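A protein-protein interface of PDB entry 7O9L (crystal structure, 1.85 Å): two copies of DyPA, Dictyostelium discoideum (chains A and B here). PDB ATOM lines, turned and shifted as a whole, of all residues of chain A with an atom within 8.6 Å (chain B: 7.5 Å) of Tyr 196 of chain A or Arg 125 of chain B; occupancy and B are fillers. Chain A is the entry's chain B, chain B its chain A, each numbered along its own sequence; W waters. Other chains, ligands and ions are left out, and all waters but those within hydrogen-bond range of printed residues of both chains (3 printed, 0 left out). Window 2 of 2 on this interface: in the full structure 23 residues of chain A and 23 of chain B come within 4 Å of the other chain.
The side-chain hydroxyl (OH) of Tyr 196 of chain A lies within hydrogen-bond range of the side-chain amide nitrogen (NE2) of Gln 121 of chain B (3.3 Å).
OE1 of Gln 121 of chain B sits at hydrogen-bond distance from NH2 of Arg 143 of chain A, at 2.9 Å.
Printed residues of chain A that touch a printed residue of chain B: Arg 143, Leu 149, Tyr 196 and Ile 252.
Of the 12 printed residues of chain B, 4 touch a printed residue of chain A.
Hydrophobic or aromatic side chains of chain B that line the printed part of chain A: Ala 120 and Met 124.
Along chain B the printed residues that touch a printed residue of chain A span positions 120 to 125.
Among the printed residues, 7 pairs touch across the chains.
Among the printed residues, no Asp or Glu carboxylate lies within 4 Å of a Lys or Arg side-chain nitrogen of the other chain.
Water W3 lies within hydrogen-bond range of OH of Tyr 196 of chain A, O of Leu 149 of chain A, NE2 of Gln 121 of chain B and OD2 of Asp 151 of chain A.
Water W2 lies within hydrogen-bond range of NE2 of Gln 121 of chain B and OH of Tyr 196 of chain A.
Water W1 bridges NH2 of Arg 143 of chain A (3.1 Å) and OE1 of Gln 121 of chain B (3.5 Å).
Among the printed residues, pairs that only touch across the chains: Leu 149 of chain A with Gln 121 of chain B, Tyr 196 of chain A with Arg 125 of chain B, Ile 252 of chain A with Ala 120 of chain B, Ile 252 of chain A with Gln 121 of chain B and Ile 252 of chain A with Met 124 of chain B.
Of the printed residues of chain B, Arg 143 of chain A touches Gln 121 (2.9 Å).
Printed residues of chain B within 4 Å of Leu 149 of chain A: Gln 121 (3.7 Å).
Tyr 196 of chain A touches just these residues of chain B: Gln 121 (3.3 Å) and Arg 125 (3.5 Å).
Of the printed residues of chain B, Ile 252 of chain A touches Ala 120, Gln 121 and Met 124.
Of the printed residues of chain A, Ala 120 of chain B touches Ile 252.
Of the printed residues of chain A, Met 124 of chain B touches Ile 252 (3.8 Å).
Arg 125 of chain B touches one residue of chain A.
The nearest printed residue of chain A that does not touch Met 124 of chain B is Thr 253 of chain A (4.4 Å).
No position is printed for both chains.
Of the 7 pairs that touch across the chains among the printed residues, none has its exchanged pair printed and touching as well.
The side-chain carboxylate (OD1) of Asp 151 of chain A is in salt-bridge range of the guanidinium group (NH2) of Arg 143 of chain A (2.8 Å).
NH1 of Arg 143 of chain A lies within hydrogen-bond range of O of Asp 148 of chain A (2.8 Å).
The backbone carbonyl oxygen of Ile 252 of chain A lies within hydrogen-bond range of the side-chain amino group of Lys 256 of chain A (2.8 Å).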
ATOM      1  N   ARG A 143     -11.929  14.208  14.531  1.00  0.00           N
ATOM      2  CA  ARG A 143     -12.399  13.641  13.277  1.00  0.00           C
ATOM      3  C   ARG A 143     -13.531  14.491  12.699  1.00  0.00           C
ATOM      4  O   ARG A 143     -14.071  15.386  13.353  1.00  0.00           O
ATOM      5  CB  ARG A 143     -12.856  12.182  13.485  1.00  0.00           C
ATOM      6  CG  ARG A 143     -11.663  11.228  13.608  1.00  0.00           C
ATOM      7  CD  ARG A 143     -12.113   9.824  14.004  1.00  0.00           C
ATOM      8  NE  ARG A 143     -12.806   9.081  12.944  1.00  0.00           N
ATOM      9  CZ  ARG A 143     -14.050   8.611  13.035  1.00  0.00           C
ATOM     10  NH1 ARG A 143     -14.778   8.874  14.111  1.00  0.00           N
ATOM     11  NH2 ARG A 143     -14.581   7.897  12.042  1.00  0.00           N
ATOM     12  N   ASP A 148     -16.366  10.460  17.765  1.00  0.00           N
ATOM     13  CA  ASP A 148     -15.534   9.390  18.300  1.00  0.00           C
ATOM     14  C   ASP A 148     -15.451   8.246  17.282  1.00  0.00           C
ATOM     15  O   ASP A 148     -16.260   8.151  16.359  1.00  0.00           O
ATOM     16  CB  ASP A 148     -16.140   8.911  19.627  1.00  0.00           C
ATOM     17  CG  ASP A 148     -15.468   7.686  20.189  1.00  0.00           C
ATOM     18  OD1 ASP A 148     -14.402   7.825  20.827  1.00  0.00           O
ATOM     19  OD2 ASP A 148     -16.029   6.578  20.029  1.00  0.00           O
ATOM     20  N   LEU A 149     -14.456   7.363  17.453  1.00  0.00           N
ATOM     21  CA  LEU A 149     -14.310   6.238  16.523  1.00  0.00           C
ATOM     22  C   LEU A 149     -15.472   5.244  16.586  1.00  0.00           C
ATOM     23  O   LEU A 149     -15.595   4.410  15.678  1.00  0.00           O
ATOM     24  CB  LEU A 149     -12.972   5.531  16.782  1.00  0.00           C
ATOM     25  CG  LEU A 149     -11.798   6.300  16.142  1.00  0.00           C
ATOM     26  CD1 LEU A 149     -10.483   5.838  16.724  1.00  0.00           C
ATOM     27  CD2 LEU A 149     -11.805   6.121  14.609  1.00  0.00           C
ATOM     28  N   THR A 150     -16.344   5.323  17.602  1.00  0.00           N
ATOM     29  CA  THR A 150     -17.640   4.639  17.516  1.00  0.00           C
ATOM     30  C   THR A 150     -18.544   5.250  16.458  1.00  0.00           C
ATOM     31  O   THR A 150     -19.589   4.665  16.141  1.00  0.00           O
ATOM     32  CB  THR A 150     -18.401   4.686  18.846  1.00  0.00           C
ATOM     33  OG1 THR A 150     -18.563   6.052  19.261  1.00  0.00           O
ATOM     34  CG2 THR A 150     -17.674   3.906  19.929  1.00  0.00           C
ATOM     35  N   ASP A 151     -18.159   6.410  15.928  1.00  0.00           N
ATOM     36  CA  ASP A 151     -18.890   7.195  14.946  1.00  0.00           C
ATOM     37  C   ASP A 151     -20.126   7.870  15.536  1.00  0.00           C
ATOM     38  O   ASP A 151     -20.992   8.335  14.789  1.00  0.00           O
ATOM     39  CB  ASP A 151     -19.229   6.365  13.704  1.00  0.00           C
ATOM     40  CG  ASP A 151     -17.977   6.056  12.878  1.00  0.00           C
ATOM     41  OD1 ASP A 151     -17.087   6.928  12.850  1.00  0.00           O
ATOM     42  OD2 ASP A 151     -17.857   4.961  12.292  1.00  0.00           O
ATOM     43  N   HIS A 190     -10.526   0.819  21.607  1.00  0.00           N
ATOM     44  CA  HIS A 190     -11.831   0.411  21.093  1.00  0.00           C
ATOM     45  C   HIS A 190     -11.732  -0.941  20.399  1.00  0.00           C
ATOM     46  O   HIS A 190     -10.761  -1.215  19.693  1.00  0.00           O
ATOM     47  CB  HIS A 190     -12.349   1.434  20.081  1.00  0.00           C
ATOM     48  CG  HIS A 190     -12.809   2.724  20.681  1.00  0.00           C
ATOM     49  ND1 HIS A 190     -12.659   3.032  22.015  1.00  0.00           N
ATOM     50  CD2 HIS A 190     -13.451   3.778  20.122  1.00  0.00           C
ATOM     51  CE1 HIS A 190     -13.160   4.232  22.247  1.00  0.00           C
ATOM     52  NE2 HIS A 190     -13.652   4.704  21.117  1.00  0.00           N
ATOM     53  N   ASN A 191     -12.749  -1.787  20.590  1.00  0.00           N
ATOM     54  CA  ASN A 191     -12.864  -3.035  19.834  1.00  0.00           C
ATOM     55  C   ASN A 191     -13.884  -2.817  18.721  1.00  0.00           C
ATOM     56  O   ASN A 191     -15.063  -3.151  18.841  1.00  0.00           O
ATOM     57  CB  ASN A 191     -13.271  -4.185  20.741  1.00  0.00           C
ATOM     58  CG  ASN A 191     -13.234  -5.532  20.033  1.00  0.00           C
ATOM     59  OD1 ASN A 191     -13.100  -5.611  18.808  1.00  0.00           O
ATOM     60  ND2 ASN A 191     -13.378  -6.599  20.806  1.00  0.00           N
ATOM     61  N   LEU A 192     -13.411  -2.255  17.609  1.00  0.00           N
ATOM     62  CA  LEU A 192     -14.341  -1.878  16.548  1.00  0.00           C
ATOM     63  C   LEU A 192     -14.797  -3.078  15.728  1.00  0.00           C
ATOM     64  O   LEU A 192     -15.883  -3.041  15.138  1.00  0.00           O
ATOM     65  CB  LEU A 192     -13.708  -0.813  15.648  1.00  0.00           C
ATOM     66  CG  LEU A 192     -13.471   0.544  16.326  1.00  0.00           C
ATOM     67  CD1 LEU A 192     -12.961   1.545  15.292  1.00  0.00           C
ATOM     68  CD2 LEU A 192     -14.739   1.060  17.010  1.00  0.00           C
ATOM     69  N   LYS A 193     -13.990  -4.146  15.675  1.00  0.00           N
ATOM     70  CA  LYS A 193     -14.471  -5.389  15.074  1.00  0.00           C
ATOM     71  C   LYS A 193     -15.731  -5.890  15.767  1.00  0.00           C
ATOM     72  O   LYS A 193     -16.582  -6.509  15.127  1.00  0.00           O
ATOM     73  CB  LYS A 193     -13.387  -6.466  15.127  1.00  0.00           C
ATOM     74  CG  LYS A 193     -12.177  -6.151  14.256  1.00  0.00           C
ATOM     75  CD  LYS A 193     -11.405  -7.418  13.893  1.00  0.00           C
ATOM     76  CE  LYS A 193     -10.533  -7.880  15.055  1.00  0.00           C
ATOM     77  NZ  LYS A 193      -9.593  -6.814  15.519  1.00  0.00           N
ATOM     78  N   LYS A 194     -15.862  -5.639  17.069  1.00  0.00           N
ATOM     79  CA  LYS A 194     -17.059  -6.049  17.797  1.00  0.00           C
ATOM     80  C   LYS A 194     -18.193  -5.042  17.640  1.00  0.00           C
ATOM     81  O   LYS A 194     -19.367  -5.429  17.604  1.00  0.00           O
ATOM     82  CB  LYS A 194     -16.710  -6.240  19.273  1.00  0.00           C
ATOM     83  CG  LYS A 194     -17.845  -6.706  20.155  1.00  0.00           C
ATOM     84  CD  LYS A 194     -17.317  -7.007  21.555  1.00  0.00           C
ATOM     85  CE  LYS A 194     -18.446  -7.402  22.505  1.00  0.00           C
ATOM     86  NZ  LYS A 194     -17.957  -7.554  23.908  1.00  0.00           N
ATOM     87  N   TRP A 195     -17.860  -3.752  17.527  1.00  0.00           N
ATOM     88  CA  TRP A 195     -18.863  -2.689  17.516  1.00  0.00           C
ATOM     89  C   TRP A 195     -19.508  -2.509  16.147  1.00  0.00           C
ATOM     90  O   TRP A 195     -20.730  -2.350  16.050  1.00  0.00           O
ATOM     91  CB  TRP A 195     -18.195  -1.398  17.956  1.00  0.00           C
ATOM     92  CG  TRP A 195     -18.990  -0.135  17.843  1.00  0.00           C
ATOM     93  CD1 TRP A 195     -18.809   0.867  16.934  1.00  0.00           C
ATOM     94  CD2 TRP A 195     -20.048   0.289  18.711  1.00  0.00           C
ATOM     95  NE1 TRP A 195     -19.700   1.896  17.181  1.00  0.00           N
ATOM     96  CE2 TRP A 195     -20.466   1.566  18.270  1.00  0.00           C
ATOM     97  CE3 TRP A 195     -20.693  -0.293  19.814  1.00  0.00           C
ATOM     98  CZ2 TRP A 195     -21.486   2.282  18.903  1.00  0.00           C
ATOM     99  CZ3 TRP A 195     -21.715   0.415  20.441  1.00  0.00           C
ATOM    100  CH2 TRP A 195     -22.098   1.694  19.983  1.00  0.00           C
ATOM    101  N   TYR A 196     -18.697  -2.493  15.088  1.00  0.00           N
ATOM    102  CA  TYR A 196     -19.213  -2.231  13.745  1.00  0.00           C
ATOM    103  C   TYR A 196     -20.379  -3.127  13.356  1.00  0.00           C
ATOM    104  O   TYR A 196     -21.357  -2.612  12.789  1.00  0.00           O
ATOM    105  CB  TYR A 196     -18.094  -2.379  12.705  1.00  0.00           C
ATOM    106  CG  TYR A 196     -17.154  -1.205  12.582  1.00  0.00           C
ATOM    107  CD1 TYR A 196     -17.502   0.063  13.044  1.00  0.00           C
ATOM    108  CD2 TYR A 196     -15.907  -1.365  11.980  1.00  0.00           C
ATOM    109  CE1 TYR A 196     -16.621   1.141  12.917  1.00  0.00           C
ATOM    110  CE2 TYR A 196     -15.027  -0.305  11.851  1.00  0.00           C
ATOM    111  CZ  TYR A 196     -15.390   0.945  12.314  1.00  0.00           C
ATOM    112  OH  TYR A 196     -14.515   1.999  12.176  1.00  0.00           O
ATOM    113  N   PRO A 197     -20.351  -4.443  13.597  1.00  0.00           N
ATOM    114  CA  PRO A 197     -21.487  -5.275  13.178  1.00  0.00           C
ATOM    115  C   PRO A 197     -22.748  -5.067  14.001  1.00  0.00           C
ATOM    116  O   PRO A 197     -23.795  -5.617  13.628  1.00  0.00           O
ATOM    117  CB  PRO A 197     -20.964  -6.713  13.348  1.00  0.00           C
ATOM    118  CG  PRO A 197     -19.522  -6.608  13.563  1.00  0.00           C
ATOM    119  CD  PRO A 197     -19.258  -5.265  14.148  1.00  0.00           C
ATOM    120  N   GLU A 198     -22.697  -4.327  15.107  1.00  0.00           N
ATOM    121  CA  GLU A 198     -23.887  -4.237  15.945  1.00  0.00           C
ATOM    122  C   GLU A 198     -24.997  -3.489  15.213  1.00  0.00           C
ATOM    123  O   GLU A 198     -24.733  -2.501  14.523  1.00  0.00           O
ATOM    124  CB  GLU A 198     -23.589  -3.545  17.276  1.00  0.00           C
ATOM    125  CG  GLU A 198     -22.667  -4.344  18.207  1.00  0.00           C
ATOM    126  CD  GLU A 198     -23.379  -5.514  18.905  1.00  0.00           C
ATOM    127  OE1 GLU A 198     -23.002  -5.856  20.047  1.00  0.00           O
ATOM    128  OE2 GLU A 198     -24.318  -6.087  18.317  1.00  0.00           O
ATOM    129  N   PRO A 199     -26.245  -3.930  15.347  1.00  0.00           N
ATOM    130  CA  PRO A 199     -27.362  -3.166  14.782  1.00  0.00           C
ATOM    131  C   PRO A 199     -27.400  -1.766  15.360  1.00  0.00           C
ATOM    132  O   PRO A 199     -26.933  -1.522  16.474  1.00  0.00           O
ATOM    133  CB  PRO A 199     -28.605  -3.967  15.204  1.00  0.00           C
ATOM    134  CG  PRO A 199     -28.084  -5.332  15.564  1.00  0.00           C
ATOM    135  CD  PRO A 199     -26.695  -5.114  16.097  1.00  0.00           C
ATOM    136  N   LEU A 200     -27.976  -0.843  14.587  1.00  0.00           N
ATOM    137  CA  LEU A 200     -28.063   0.553  15.031  1.00  0.00           C
ATOM    138  C   LEU A 200     -28.809   0.686  16.358  1.00  0.00           C
ATOM    139  O   LEU A 200     -28.440   1.507  17.205  1.00  0.00           O
ATOM    140  CB  LEU A 200     -28.743   1.406  13.960  1.00  0.00           C
ATOM    141  CG  LEU A 200     -28.890   2.896  14.285  1.00  0.00           C
ATOM    142  CD1 LEU A 200     -27.520   3.566  14.416  1.00  0.00           C
ATOM    143  CD2 LEU A 200     -29.730   3.592  13.235  1.00  0.00           C
ATOM    144  N   GLN A 203     -26.392   0.012  19.060  1.00  0.00           N
ATOM    145  CA  GLN A 203     -25.437   1.107  19.247  1.00  0.00           C
ATOM    146  C   GLN A 203     -26.093   2.291  19.952  1.00  0.00           C
ATOM    147  O   GLN A 203     -25.503   2.893  20.857  1.00  0.00           O
ATOM    148  CB  GLN A 203     -24.849   1.535  17.900  1.00  0.00           C
ATOM    149  CG  GLN A 203     -24.021   0.418  17.203  1.00  0.00           C
ATOM    150  CD  GLN A 203     -23.254   0.936  16.005  1.00  0.00           C
ATOM    151  OE1 GLN A 203     -23.484   2.057  15.551  1.00  0.00           O
ATOM    152  NE2 GLN A 203     -22.319   0.126  15.493  1.00  0.00           N
ATOM    153  N   LYS A 211     -27.383   8.135  16.516  1.00  0.00           N
ATOM    154  CA  LYS A 211     -26.061   8.152  15.887  1.00  0.00           C
ATOM    155  C   LYS A 211     -25.915   9.332  14.938  1.00  0.00           C
ATOM    156  O   LYS A 211     -24.915  10.060  14.985  1.00  0.00           O
ATOM    157  CB  LYS A 211     -25.820   6.837  15.142  1.00  0.00           C
ATOM    158  CG  LYS A 211     -24.368   6.635  14.702  1.00  0.00           C
ATOM    159  CD  LYS A 211     -24.109   5.190  14.253  1.00  0.00           C
ATOM    160  CE  LYS A 211     -22.619   5.008  13.928  1.00  0.00           C
ATOM    161  NZ  LYS A 211     -22.239   3.586  13.623  1.00  0.00           N
ATOM    162  N   ILE A 252      -5.732   3.373  11.747  1.00  0.00           N
ATOM    163  CA  ILE A 252      -6.873   2.714  11.104  1.00  0.00           C
ATOM    164  C   ILE A 252      -6.706   1.205  11.144  1.00  0.00           C
ATOM    165  O   ILE A 252      -7.654   0.456  11.429  1.00  0.00           O
ATOM    166  CB  ILE A 252      -7.015   3.208   9.652  1.00  0.00           C
ATOM    167  CG1 ILE A 252      -7.376   4.691   9.626  1.00  0.00           C
ATOM    168  CG2 ILE A 252      -8.037   2.369   8.879  1.00  0.00           C
ATOM    169  CD1 ILE A 252      -6.895   5.374   8.370  1.00  0.00           C
ATOM    170  N   THR A 253      -5.498   0.734  10.859  1.00  0.00           N
ATOM    171  CA  THR A 253      -5.215  -0.685  10.737  1.00  0.00           C
ATOM    172  C   THR A 253      -4.564  -1.257  11.984  1.00  0.00           C
ATOM    173  O   THR A 253      -4.040  -2.372  11.939  1.00  0.00           O
ATOM    174  CB  THR A 253      -4.326  -0.933   9.516  1.00  0.00           C
ATOM    175  OG1 THR A 253      -3.077  -0.244   9.673  1.00  0.00           O
ATOM    176  CG2 THR A 253      -5.018  -0.425   8.268  1.00  0.00           C
ATOM    177  N   LYS A 256      -6.477   1.663  18.234  1.00  0.00           N
ATOM    178  CA  LYS A 256      -7.087   2.983  18.180  1.00  0.00           C
ATOM    179  C   LYS A 256      -8.145   3.080  19.269  1.00  0.00           C
ATOM    180  O   LYS A 256      -8.621   2.068  19.792  1.00  0.00           O
ATOM    181  CB  LYS A 256      -7.721   3.244  16.807  1.00  0.00           C
ATOM    182  CG  LYS A 256      -8.783   2.221  16.426  1.00  0.00           C
ATOM    183  CD  LYS A 256      -9.178   2.357  14.960  1.00  0.00           C
ATOM    184  CE  LYS A 256      -9.557   1.012  14.350  1.00  0.00           C
ATOM    185  NZ  LYS A 256      -8.378   0.123  14.084  1.00  0.00           N
ATOM    186  N   TYR A 291     -17.441  -2.693  24.542  1.00  0.00           N
ATOM    187  CA  TYR A 291     -16.811  -2.445  23.251  1.00  0.00           C
ATOM    188  C   TYR A 291     -15.483  -1.716  23.352  1.00  0.00           C
ATOM    189  O   TYR A 291     -14.812  -1.539  22.326  1.00  0.00           O
ATOM    190  CB  TYR A 291     -17.749  -1.630  22.355  1.00  0.00           C
ATOM    191  CG  TYR A 291     -19.087  -2.302  22.201  1.00  0.00           C
ATOM    192  CD1 TYR A 291     -19.238  -3.416  21.385  1.00  0.00           C
ATOM    193  CD2 TYR A 291     -20.194  -1.827  22.886  1.00  0.00           C
ATOM    194  CE1 TYR A 291     -20.477  -4.044  21.253  1.00  0.00           C
ATOM    195  CE2 TYR A 291     -21.420  -2.438  22.767  1.00  0.00           C
ATOM    196  CZ  TYR A 291     -21.562  -3.534  21.952  1.00  0.00           C
ATOM    197  OH  TYR A 291     -22.805  -4.108  21.861  1.00  0.00           O
ATOM    198  N   ASN B  42     -13.912  -0.953  -5.556  1.00  0.00           N
ATOM    199  CA  ASN B  42     -13.403  -0.170  -4.433  1.00  0.00           C
ATOM    200  C   ASN B  42     -12.449   0.928  -4.898  1.00  0.00           C
ATOM    201  O   ASN B  42     -12.412   2.017  -4.309  1.00  0.00           O
ATOM    202  CB  ASN B  42     -12.721  -1.102  -3.428  1.00  0.00           C
ATOM    203  CG  ASN B  42     -13.720  -1.925  -2.630  1.00  0.00           C
ATOM    204  OD1 ASN B  42     -14.805  -1.449  -2.310  1.00  0.00           O
ATOM    205  ND2 ASN B  42     -13.356  -3.160  -2.304  1.00  0.00           N
ATOM    206  N   LEU B 119     -10.864   9.976   4.506  1.00  0.00           N
ATOM    207  CA  LEU B 119     -10.683   9.263   3.241  1.00  0.00           C
ATOM    208  C   LEU B 119      -9.880   7.983   3.442  1.00  0.00           C
ATOM    209  O   LEU B 119     -10.220   6.940   2.871  1.00  0.00           O
ATOM    210  CB  LEU B 119     -10.009  10.172   2.203  1.00  0.00           C
ATOM    211  CG  LEU B 119      -9.741   9.532   0.827  1.00  0.00           C
ATOM    212  CD1 LEU B 119     -11.058   9.092   0.154  1.00  0.00           C
ATOM    213  CD2 LEU B 119      -8.965  10.505  -0.060  1.00  0.00           C
ATOM    214  N   ALA B 120      -8.812   8.034   4.251  1.00  0.00           N
ATOM    215  CA  ALA B 120      -8.021   6.822   4.490  1.00  0.00           C
ATOM    216  C   ALA B 120      -8.849   5.745   5.180  1.00  0.00           C
ATOM    217  O   ALA B 120      -8.787   4.558   4.811  1.00  0.00           O
ATOM    218  CB  ALA B 120      -6.772   7.160   5.319  1.00  0.00           C
ATOM    219  N   GLN B 121      -9.629   6.128   6.191  1.00  0.00           N
ATOM    220  CA  GLN B 121     -10.402   5.132   6.926  1.00  0.00           C
ATOM    221  C   GLN B 121     -11.530   4.562   6.074  1.00  0.00           C
ATOM    222  O   GLN B 121     -11.757   3.344   6.062  1.00  0.00           O
ATOM    223  CB  GLN B 121     -10.957   5.742   8.220  1.00  0.00           C
ATOM    224  CG  GLN B 121     -11.649   4.701   9.089  1.00  0.00           C
ATOM    225  CD  GLN B 121     -12.381   5.306  10.282  1.00  0.00           C
ATOM    226  OE1 GLN B 121     -12.831   6.453  10.244  1.00  0.00           O
ATOM    227  NE2 GLN B 121     -12.519   4.519  11.341  1.00  0.00           N
ATOM    228  N   ASP B 122     -12.274   5.428   5.377  1.00  0.00           N
ATOM    229  CA  ASP B 122     -13.349   4.946   4.512  1.00  0.00           C
ATOM    230  C   ASP B 122     -12.814   3.995   3.450  1.00  0.00           C
ATOM    231  O   ASP B 122     -13.444   2.973   3.126  1.00  0.00           O
ATOM    232  CB  ASP B 122     -14.053   6.123   3.838  1.00  0.00           C
ATOM    233  CG  ASP B 122     -14.935   6.924   4.802  1.00  0.00           C
ATOM    234  OD1 ASP B 122     -15.102   6.518   5.975  1.00  0.00           O
ATOM    235  OD2 ASP B 122     -15.460   7.975   4.374  1.00  0.00           O
ATOM    236  N   THR B 123     -11.655   4.325   2.889  1.00  0.00           N
ATOM    237  CA  THR B 123     -11.060   3.493   1.853  1.00  0.00           C
ATOM    238  C   THR B 123     -10.663   2.128   2.402  1.00  0.00           C
ATOM    239  O   THR B 123     -10.941   1.090   1.784  1.00  0.00           O
ATOM    240  CB  THR B 123      -9.852   4.225   1.256  1.00  0.00           C
ATOM    241  OG1 THR B 123     -10.298   5.470   0.693  1.00  0.00           O
ATOM    242  CG2 THR B 123      -9.216   3.392   0.163  1.00  0.00           C
ATOM    243  N   MET B 124     -10.014   2.104   3.571  1.00  0.00           N
ATOM    244  CA  MET B 124      -9.621   0.826   4.162  1.00  0.00           C
ATOM    245  C   MET B 124     -10.834  -0.010   4.545  1.00  0.00           C
ATOM    246  O   MET B 124     -10.803  -1.246   4.443  1.00  0.00           O
ATOM    247  CB  MET B 124      -8.734   1.052   5.382  1.00  0.00           C
ATOM    248  CG  MET B 124      -7.309   1.503   5.063  1.00  0.00           C
ATOM    249  SD  MET B 124      -6.478   0.328   3.978  1.00  0.00           S
ATOM    250  CE  MET B 124      -6.710   1.106   2.408  1.00  0.00           C
ATOM    251  N   ARG B 125     -11.910   0.634   4.999  1.00  0.00           N
ATOM    252  CA  ARG B 125     -13.123  -0.137   5.284  1.00  0.00           C
ATOM    253  C   ARG B 125     -13.781  -0.662   4.016  1.00  0.00           C
ATOM    254  O   ARG B 125     -14.414  -1.728   4.045  1.00  0.00           O
ATOM    255  CB  ARG B 125     -14.111   0.704   6.091  1.00  0.00           C
ATOM    256  CG  ARG B 125     -13.681   0.867   7.543  1.00  0.00           C
ATOM    257  CD  ARG B 125     -14.770   1.468   8.395  1.00  0.00           C
ATOM    258  NE  ARG B 125     -15.911   0.566   8.551  1.00  0.00           N
ATOM    259  CZ  ARG B 125     -17.132   0.965   8.903  1.00  0.00           C
ATOM    260  NH1 ARG B 125     -17.370   2.251   9.139  1.00  0.00           N
ATOM    261  NH2 ARG B 125     -18.116   0.084   9.022  1.00  0.00           N
ATOM    262  N   ASN B 126     -13.666   0.056   2.898  1.00  0.00           N
ATOM    263  CA  ASN B 126     -14.225  -0.457   1.648  1.00  0.00           C
ATOM    264  C   ASN B 126     -13.461  -1.688   1.167  1.00  0.00           C
ATOM    265  O   ASN B 126     -14.066  -2.716   0.838  1.00  0.00           O
ATOM    266  CB  ASN B 126     -14.206   0.622   0.565  1.00  0.00           C
ATOM    267  CG  ASN B 126     -15.321   1.616   0.713  1.00  0.00           C
ATOM    268  OD1 ASN B 126     -16.324   1.335   1.349  1.00  0.00           O
ATOM    269  ND2 ASN B 126     -15.154   2.791   0.116  1.00  0.00           N
ATOM    270  N   PHE B 127     -12.130  -1.589   1.087  1.00  0.00           N
ATOM    271  CA  PHE B 127     -11.319  -2.733   0.669  1.00  0.00           C
ATOM    272  C   PHE B 127     -11.413  -3.867   1.681  1.00  0.00           C
ATOM    273  O   PHE B 127     -11.654  -5.021   1.312  1.00  0.00           O
ATOM    274  CB  PHE B 127      -9.854  -2.320   0.486  1.00  0.00           C
ATOM    275  CG  PHE B 127      -9.591  -1.550  -0.773  1.00  0.00           C
ATOM    276  CD1 PHE B 127      -9.527  -2.194  -1.996  1.00  0.00           C
ATOM    277  CD2 PHE B 127      -9.395  -0.176  -0.729  1.00  0.00           C
ATOM    278  CE1 PHE B 127      -9.274  -1.484  -3.161  1.00  0.00           C
ATOM    279  CE2 PHE B 127      -9.147   0.540  -1.886  1.00  0.00           C
ATOM    280  CZ  PHE B 127      -9.092  -0.115  -3.106  1.00  0.00           C
ATOM    281  N   GLY B 128     -11.206  -3.560   2.960  1.00  0.00           N
ATOM    282  CA  GLY B 128     -11.343  -4.537   4.018  1.00  0.00           C
ATOM    283  C   GLY B 128     -10.115  -5.417   4.168  1.00  0.00           C
ATOM    284  O   GLY B 128      -9.241  -5.485   3.304  1.00  0.00           O
ATOM    285  N   GLU B 129     -10.061  -6.118   5.302  1.00  0.00           N
ATOM    286  CA  GLU B 129      -8.981  -7.061   5.560  1.00  0.00           C
ATOM    287  C   GLU B 129      -9.063  -8.302   4.682  1.00  0.00           C
ATOM    288  O   GLU B 129      -8.099  -9.072   4.641  1.00  0.00           O
ATOM    289  CB  GLU B 129      -8.977  -7.476   7.033  1.00  0.00           C
ATOM    290  CG  GLU B 129      -9.255  -6.337   8.002  1.00  0.00           C
ATOM    291  CD  GLU B 129     -10.741  -6.150   8.282  1.00  0.00           C
ATOM    292  OE1 GLU B 129     -11.183  -6.483   9.403  1.00  0.00           O
ATOM    293  OE2 GLU B 129     -11.466  -5.669   7.383  1.00  0.00           O
HETATM  294  O   HOH W   1     -13.345   9.891   9.956  1.00  0.00           O
HETATM  295  O   HOH W   2     -11.691   1.709  11.234  1.00  0.00           O
HETATM  296  O   HOH W   3     -14.935   4.326  13.089  1.00  0.00           O
